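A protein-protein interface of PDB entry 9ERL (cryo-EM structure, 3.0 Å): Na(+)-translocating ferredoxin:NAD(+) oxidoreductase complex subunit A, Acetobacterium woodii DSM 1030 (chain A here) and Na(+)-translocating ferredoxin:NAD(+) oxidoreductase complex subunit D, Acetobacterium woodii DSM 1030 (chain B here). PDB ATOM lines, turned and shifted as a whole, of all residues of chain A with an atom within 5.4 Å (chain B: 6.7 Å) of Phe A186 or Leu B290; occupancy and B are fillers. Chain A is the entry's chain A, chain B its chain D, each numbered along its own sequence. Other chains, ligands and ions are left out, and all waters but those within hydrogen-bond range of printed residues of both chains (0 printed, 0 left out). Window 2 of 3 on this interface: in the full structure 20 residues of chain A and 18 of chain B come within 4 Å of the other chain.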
ATOM      1  N   PHE A  12       7.885 -16.246  24.038  1.00  0.00           N
ATOM      2  CA  PHE A  12       8.969 -16.508  23.095  1.00  0.00           C
ATOM      3  C   PHE A  12       8.886 -15.652  21.831  1.00  0.00           C
ATOM      4  O   PHE A  12       9.822 -14.913  21.515  1.00  0.00           O
ATOM      5  CB  PHE A  12       8.983 -17.995  22.724  1.00  0.00           C
ATOM      6  CG  PHE A  12       9.474 -18.887  23.825  1.00  0.00           C
ATOM      7  CD1 PHE A  12      10.811 -18.897  24.181  1.00  0.00           C
ATOM      8  CD2 PHE A  12       8.597 -19.709  24.510  1.00  0.00           C
ATOM      9  CE1 PHE A  12      11.267 -19.714  25.194  1.00  0.00           C
ATOM     10  CE2 PHE A  12       9.046 -20.528  25.527  1.00  0.00           C
ATOM     11  CZ  PHE A  12      10.383 -20.530  25.868  1.00  0.00           C
ATOM     12  N   VAL A  13       7.777 -15.759  21.095  1.00  0.00           N
ATOM     13  CA  VAL A  13       7.700 -15.160  19.764  1.00  0.00           C
ATOM     14  C   VAL A  13       7.681 -13.638  19.843  1.00  0.00           C
ATOM     15  O   VAL A  13       8.273 -12.953  19.001  1.00  0.00           O
ATOM     16  CB  VAL A  13       6.474 -15.704  19.009  1.00  0.00           C
ATOM     17  CG1 VAL A  13       6.551 -15.339  17.536  1.00  0.00           C
ATOM     18  CG2 VAL A  13       6.375 -17.211  19.178  1.00  0.00           C
ATOM     19  N   ALA A 182      19.674 -13.130  17.908  1.00  0.00           N
ATOM     20  CA  ALA A 182      19.360 -14.530  18.187  1.00  0.00           C
ATOM     21  C   ALA A 182      17.859 -14.746  18.342  1.00  0.00           C
ATOM     22  O   ALA A 182      17.325 -15.776  17.915  1.00  0.00           O
ATOM     23  CB  ALA A 182      20.101 -14.998  19.437  1.00  0.00           C
ATOM     24  N   PHE A 183      17.158 -13.783  18.948  1.00  0.00           N
ATOM     25  CA  PHE A 183      15.704 -13.874  19.043  1.00  0.00           C
ATOM     26  C   PHE A 183      14.992 -13.471  17.756  1.00  0.00           C
ATOM     27  O   PHE A 183      13.840 -13.866  17.558  1.00  0.00           O
ATOM     28  CB  PHE A 183      15.192 -13.023  20.203  1.00  0.00           C
ATOM     29  CG  PHE A 183      14.909 -13.811  21.447  1.00  0.00           C
ATOM     30  CD1 PHE A 183      15.943 -14.374  22.176  1.00  0.00           C
ATOM     31  CD2 PHE A 183      13.610 -14.003  21.881  1.00  0.00           C
ATOM     32  CE1 PHE A 183      15.686 -15.104  23.317  1.00  0.00           C
ATOM     33  CE2 PHE A 183      13.346 -14.733  23.022  1.00  0.00           C
ATOM     34  CZ  PHE A 183      14.386 -15.284  23.741  1.00  0.00           C
ATOM     35  N   LEU A 184      15.640 -12.684  16.890  1.00  0.00           N
ATOM     36  CA  LEU A 184      15.100 -12.442  15.554  1.00  0.00           C
ATOM     37  C   LEU A 184      15.037 -13.734  14.764  1.00  0.00           C
ATOM     38  O   LEU A 184      14.211 -13.882  13.856  1.00  0.00           O
ATOM     39  CB  LEU A 184      15.950 -11.417  14.805  1.00  0.00           C
ATOM     40  CG  LEU A 184      15.317 -10.081  14.422  1.00  0.00           C
ATOM     41  CD1 LEU A 184      16.149  -9.413  13.344  1.00  0.00           C
ATOM     42  CD2 LEU A 184      13.885 -10.267  13.955  1.00  0.00           C
ATOM     43  N   GLY A 185      15.919 -14.678  15.086  1.00  0.00           N
ATOM     44  CA  GLY A 185      15.752 -16.024  14.557  1.00  0.00           C
ATOM     45  C   GLY A 185      14.446 -16.674  14.983  1.00  0.00           C
ATOM     46  O   GLY A 185      13.911 -17.534  14.280  1.00  0.00           O
ATOM     47  N   PHE A 186      13.918 -16.276  16.142  1.00  0.00           N
ATOM     48  CA  PHE A 186      12.697 -16.856  16.710  1.00  0.00           C
ATOM     49  C   PHE A 186      11.493 -16.025  16.271  1.00  0.00           C
ATOM     50  O   PHE A 186      10.839 -15.347  17.067  1.00  0.00           O
ATOM     51  CB  PHE A 186      12.802 -16.908  18.231  1.00  0.00           C
ATOM     52  CG  PHE A 186      12.278 -18.172  18.836  1.00  0.00           C
ATOM     53  CD1 PHE A 186      11.137 -18.776  18.342  1.00  0.00           C
ATOM     54  CD2 PHE A 186      12.931 -18.756  19.907  1.00  0.00           C
ATOM     55  CE1 PHE A 186      10.660 -19.941  18.903  1.00  0.00           C
ATOM     56  CE2 PHE A 186      12.461 -19.920  20.471  1.00  0.00           C
ATOM     57  CZ  PHE A 186      11.323 -20.515  19.969  1.00  0.00           C
ATOM     58  N   SER A 187      11.186 -16.091  14.978  1.00  0.00           N
ATOM     59  CA  SER A 187      10.136 -15.245  14.421  1.00  0.00           C
ATOM     60  C   SER A 187       9.539 -15.923  13.198  1.00  0.00           C
ATOM     61  O   SER A 187      10.113 -16.857  12.635  1.00  0.00           O
ATOM     62  CB  SER A 187      10.667 -13.854  14.060  1.00  0.00           C
ATOM     63  OG  SER A 187      11.026 -13.786  12.692  1.00  0.00           O
ATOM     64  N   GLY A 188       8.372 -15.429  12.792  1.00  0.00           N
ATOM     65  CA  GLY A 188       7.654 -15.964  11.657  1.00  0.00           C
ATOM     66  C   GLY A 188       6.732 -17.121  11.968  1.00  0.00           C
ATOM     67  O   GLY A 188       5.991 -17.555  11.078  1.00  0.00           O
ATOM     68  N   MET A 189       6.747 -17.629  13.198  1.00  0.00           N
ATOM     69  CA  MET A 189       5.883 -18.738  13.577  1.00  0.00           C
ATOM     70  C   MET A 189       4.441 -18.267  13.695  1.00  0.00           C
ATOM     71  O   MET A 189       4.168 -17.214  14.280  1.00  0.00           O
ATOM     72  CB  MET A 189       6.343 -19.350  14.900  1.00  0.00           C
ATOM     73  CG  MET A 189       7.549 -20.259  14.779  1.00  0.00           C
ATOM     74  SD  MET A 189       7.669 -21.424  16.146  1.00  0.00           S
ATOM     75  CE  MET A 189       9.414 -21.813  16.097  1.00  0.00           C
ATOM     76  N   ILE B 270      15.502 -27.546  19.220  1.00  0.00           N
ATOM     77  CA  ILE B 270      15.150 -26.275  18.589  1.00  0.00           C
ATOM     78  C   ILE B 270      15.301 -26.360  17.071  1.00  0.00           C
ATOM     79  O   ILE B 270      14.514 -25.758  16.326  1.00  0.00           O
ATOM     80  CB  ILE B 270      15.979 -25.125  19.191  1.00  0.00           C
ATOM     81  CG1 ILE B 270      15.734 -25.025  20.695  1.00  0.00           C
ATOM     82  CG2 ILE B 270      15.620 -23.798  18.546  1.00  0.00           C
ATOM     83  CD1 ILE B 270      16.613 -24.012  21.390  1.00  0.00           C
ATOM     84  N   ILE B 273      12.137 -28.008  15.813  1.00  0.00           N
ATOM     85  CA  ILE B 273      10.981 -27.137  16.017  1.00  0.00           C
ATOM     86  C   ILE B 273      10.937 -26.033  14.965  1.00  0.00           C
ATOM     87  O   ILE B 273       9.878 -25.756  14.389  1.00  0.00           O
ATOM     88  CB  ILE B 273      10.980 -26.565  17.448  1.00  0.00           C
ATOM     89  CG1 ILE B 273      10.625 -27.656  18.458  1.00  0.00           C
ATOM     90  CG2 ILE B 273      10.002 -25.409  17.572  1.00  0.00           C
ATOM     91  CD1 ILE B 273      10.918 -27.277  19.887  1.00  0.00           C
ATOM     92  N   ILE B 274      12.076 -25.394  14.680  1.00  0.00           N
ATOM     93  CA  ILE B 274      12.100 -24.386  13.620  1.00  0.00           C
ATOM     94  C   ILE B 274      11.913 -24.999  12.233  1.00  0.00           C
ATOM     95  O   ILE B 274      11.254 -24.391  11.381  1.00  0.00           O
ATOM     96  CB  ILE B 274      13.396 -23.557  13.677  1.00  0.00           C
ATOM     97  CG1 ILE B 274      13.575 -22.952  15.071  1.00  0.00           C
ATOM     98  CG2 ILE B 274      13.382 -22.449  12.635  1.00  0.00           C
ATOM     99  CD1 ILE B 274      14.678 -21.920  15.160  1.00  0.00           C
ATOM    100  N   TYR B 280      11.246 -20.691   8.411  1.00  0.00           N
ATOM    101  CA  TYR B 280      12.469 -20.949   7.669  1.00  0.00           C
ATOM    102  C   TYR B 280      12.503 -22.406   7.235  1.00  0.00           C
ATOM    103  O   TYR B 280      11.910 -23.265   7.894  1.00  0.00           O
ATOM    104  CB  TYR B 280      13.717 -20.653   8.516  1.00  0.00           C
ATOM    105  CG  TYR B 280      13.834 -19.235   9.029  1.00  0.00           C
ATOM    106  CD1 TYR B 280      14.413 -18.241   8.255  1.00  0.00           C
ATOM    107  CD2 TYR B 280      13.389 -18.898  10.300  1.00  0.00           C
ATOM    108  CE1 TYR B 280      14.528 -16.948   8.724  1.00  0.00           C
ATOM    109  CE2 TYR B 280      13.501 -17.609  10.775  1.00  0.00           C
ATOM    110  CZ  TYR B 280      14.071 -16.638   9.984  1.00  0.00           C
ATOM    111  OH  TYR B 280      14.185 -15.353  10.458  1.00  0.00           O
ATOM    112  N   SER B 285      21.263 -22.666  12.479  1.00  0.00           N
ATOM    113  CA  SER B 285      22.044 -21.514  12.915  1.00  0.00           C
ATOM    114  C   SER B 285      21.431 -20.851  14.142  1.00  0.00           C
ATOM    115  O   SER B 285      22.134 -20.533  15.108  1.00  0.00           O
ATOM    116  CB  SER B 285      22.165 -20.511  11.767  1.00  0.00           C
ATOM    117  OG  SER B 285      22.373 -19.199  12.255  1.00  0.00           O
ATOM    118  N   TYR B 286      20.113 -20.656  14.131  1.00  0.00           N
ATOM    119  CA  TYR B 286      19.459 -20.009  15.264  1.00  0.00           C
ATOM    120  C   TYR B 286      19.361 -20.935  16.468  1.00  0.00           C
ATOM    121  O   TYR B 286      19.375 -20.460  17.608  1.00  0.00           O
ATOM    122  CB  TYR B 286      18.078 -19.509  14.852  1.00  0.00           C
ATOM    123  CG  TYR B 286      18.117 -18.564  13.676  1.00  0.00           C
ATOM    124  CD1 TYR B 286      18.815 -17.367  13.752  1.00  0.00           C
ATOM    125  CD2 TYR B 286      17.470 -18.871  12.489  1.00  0.00           C
ATOM    126  CE1 TYR B 286      18.855 -16.497  12.686  1.00  0.00           C
ATOM    127  CE2 TYR B 286      17.510 -18.008  11.414  1.00  0.00           C
ATOM    128  CZ  TYR B 286      18.204 -16.822  11.519  1.00  0.00           C
ATOM    129  OH  TYR B 286      18.249 -15.956  10.454  1.00  0.00           O
ATOM    130  N   SER B 287      19.262 -22.248  16.244  1.00  0.00           N
ATOM    131  CA  SER B 287      19.284 -23.185  17.363  1.00  0.00           C
ATOM    132  C   SER B 287      20.638 -23.179  18.056  1.00  0.00           C
ATOM    133  O   SER B 287      20.713 -23.268  19.286  1.00  0.00           O
ATOM    134  CB  SER B 287      18.937 -24.594  16.886  1.00  0.00           C
ATOM    135  OG  SER B 287      20.042 -25.200  16.244  1.00  0.00           O
ATOM    136  N   ILE B 288      21.723 -23.088  17.283  1.00  0.00           N
ATOM    137  CA  ILE B 288      23.043 -22.994  17.900  1.00  0.00           C
ATOM    138  C   ILE B 288      23.246 -21.637  18.572  1.00  0.00           C
ATOM    139  O   ILE B 288      23.794 -21.568  19.677  1.00  0.00           O
ATOM    140  CB  ILE B 288      24.144 -23.287  16.865  1.00  0.00           C
ATOM    141  CG1 ILE B 288      24.034 -24.732  16.374  1.00  0.00           C
ATOM    142  CG2 ILE B 288      25.521 -23.055  17.459  1.00  0.00           C
ATOM    143  CD1 ILE B 288      24.910 -25.039  15.188  1.00  0.00           C
ATOM    144  N   LEU B 289      22.804 -20.543  17.942  1.00  0.00           N
ATOM    145  CA  LEU B 289      22.954 -19.218  18.536  1.00  0.00           C
ATOM    146  C   LEU B 289      22.124 -19.031  19.799  1.00  0.00           C
ATOM    147  O   LEU B 289      22.538 -18.276  20.684  1.00  0.00           O
ATOM    148  CB  LEU B 289      22.580 -18.129  17.529  1.00  0.00           C
ATOM    149  CG  LEU B 289      23.559 -17.817  16.399  1.00  0.00           C
ATOM    150  CD1 LEU B 289      22.926 -16.852  15.414  1.00  0.00           C
ATOM    151  CD2 LEU B 289      24.852 -17.249  16.949  1.00  0.00           C
ATOM    152  N   LEU B 290      20.965 -19.683  19.901  1.00  0.00           N
ATOM    153  CA  LEU B 290      20.144 -19.568  21.100  1.00  0.00           C
ATOM    154  C   LEU B 290      20.713 -20.343  22.279  1.00  0.00           C
ATOM    155  O   LEU B 290      20.401 -20.012  23.427  1.00  0.00           O
ATOM    156  CB  LEU B 290      18.719 -20.047  20.816  1.00  0.00           C
ATOM    157  CG  LEU B 290      17.755 -19.009  20.241  1.00  0.00           C
ATOM    158  CD1 LEU B 290      16.541 -19.683  19.634  1.00  0.00           C
ATOM    159  CD2 LEU B 290      17.339 -18.020  21.314  1.00  0.00           C
ATOM    160  N   MET B 291      21.526 -21.367  22.027  1.00  0.00           N
ATOM    161  CA  MET B 291      22.167 -22.134  23.084  1.00  0.00           C
ATOM    162  C   MET B 291      23.515 -21.562  23.496  1.00  0.00           C
ATOM    163  O   MET B 291      24.106 -22.043  24.467  1.00  0.00           O
ATOM    164  CB  MET B 291      22.328 -23.593  22.653  1.00  0.00           C
ATOM    165  CG  MET B 291      21.041 -24.395  22.726  1.00  0.00           C
ATOM    166  SD  MET B 291      20.626 -24.886  24.408  1.00  0.00           S
ATOM    167  CE  MET B 291      18.910 -24.387  24.491  1.00  0.00           C
ATOM    168  N   ASN B 292      24.020 -20.560  22.779  1.00  0.00           N
ATOM    169  CA  ASN B 292      25.162 -19.777  23.230  1.00  0.00           C
ATOM    170  C   ASN B 292      24.774 -18.728  24.259  1.00  0.00           C
ATOM    171  O   ASN B 292      25.649 -18.213  24.961  1.00  0.00           O
ATOM    172  CB  ASN B 292      25.840 -19.088  22.040  1.00  0.00           C
ATOM    173  CG  ASN B 292      26.553 -20.062  21.131  1.00  0.00           C
ATOM    174  OD1 ASN B 292      26.725 -21.231  21.468  1.00  0.00           O
ATOM    175  ND2 ASN B 292      26.973 -19.584  19.969  1.00  0.00           N
ATOM    176  N   VAL B 293      23.486 -18.407  24.362  1.00  0.00           N
ATOM    177  CA  VAL B 293      23.007 -17.455  25.353  1.00  0.00           C
ATOM    178  C   VAL B 293      22.716 -18.141  26.686  1.00  0.00           C
ATOM    179  O   VAL B 293      23.032 -17.594  27.748  1.00  0.00           O
ATOM    180  CB  VAL B 293      21.765 -16.726  24.806  1.00  0.00           C
ATOM    181  CG1 VAL B 293      21.037 -15.966  25.899  1.00  0.00           C
ATOM    182  CG2 VAL B 293      22.156 -15.791  23.670  1.00  0.00           C
ATOM    183  N   ALA B 294      22.145 -19.344  26.654  1.00  0.00           N
ATOM    184  CA  ALA B 294      21.804 -20.084  27.859  1.00  0.00           C
ATOM    185  C   ALA B 294      22.973 -20.868  28.440  1.00  0.00           C
ATOM    186  O   ALA B 294      22.807 -21.500  29.488  1.00  0.00           O
ATOM    187  CB  ALA B 294      20.647 -21.045  27.574  1.00  0.00           C
ATOM    188  N   THR B 295      24.135 -20.856  27.785  1.00  0.00           N
ATOM    189  CA  THR B 295      25.288 -21.607  28.283  1.00  0.00           C
ATOM    190  C   THR B 295      25.775 -21.143  29.656  1.00  0.00           C
ATOM    191  O   THR B 295      26.053 -22.012  30.502  1.00  0.00           O
ATOM    192  CB  THR B 295      26.408 -21.583  27.235  1.00  0.00           C
ATOM    193  OG1 THR B 295      26.015 -22.363  26.100  1.00  0.00           O
ATOM    194  CG2 THR B 295      27.695 -22.151  27.799  1.00  0.00           C
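O of Leu A184 is in hydrogen-bond range of OG of Ser A187 (3.4 Å).
CD2 of Leu B290 touches CE1 of Phe A183 (3.9 Å).
Leu A184 touches Tyr B280 (O to OH, 3.7 Å).
O of Gly A185 touches CE2 of Tyr B280, 3.5 Å away.
Gly A185 touches Tyr B286 (CA to CD1, 3.4 Å).
Leu B290 touches Phe A186 (CD1 to CD2, 3.7 Å).
O of Ser A187 touches CE2 of Tyr B280 (3.9 Å).
Met A189 touches Ile B273 (CE to CG2, 3.9 Å).
Phe A186 touches just one residue of chain B: Leu B290 (3.7 Å).
Of the printed residues of chain B, Phe A183 touches Leu B290 (3.9 Å).
Of the printed residues of chain B, Leu A184 touches Tyr B280 (3.7 Å).
Printed residues of chain B within 4 Å of Ser A187: Tyr B280 (3.9 Å).
Of the printed residues of chain A, Ile B273 touches Met A189 (3.9 Å).
Of the printed residues of chain B, Gly A185 touches Tyr B280 (3.5 Å) and Tyr B286 (3.4 Å).
Ile B274 touches none of the printed residues of chain A.
Val B293 touches none of the printed residues of chain A.
The nearest printed residue of chain A that does not touch Leu B290 is Ala A182 (4.01 Å).
The nearest printed residue of chain A that does not touch Ile B273 is Phe A186 (5.6 Å).
Printed residues of chain B that touch a printed residue of chain A: Ile B273, Tyr B280, Tyr B286 and Leu B290.
Hydrophobic or aromatic side chains of chain B within 4 Å of the printed part of chain A: Ile B273, Tyr B280, Tyr B286 and Leu B290.
Of the 10 printed residues of chain A, 6 touch a printed residue of chain B.
Hydrophobic or aromatic side chains of chain A that line the printed part of chain B: Phe A183, Phe A186 and Met A189.
Among the printed residues, 7 pairs touch across the chains.
Among the printed residues, no Asp or Glu carboxylate lies within 4 Å of a Lys or Arg side-chain nitrogen of the other chain.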
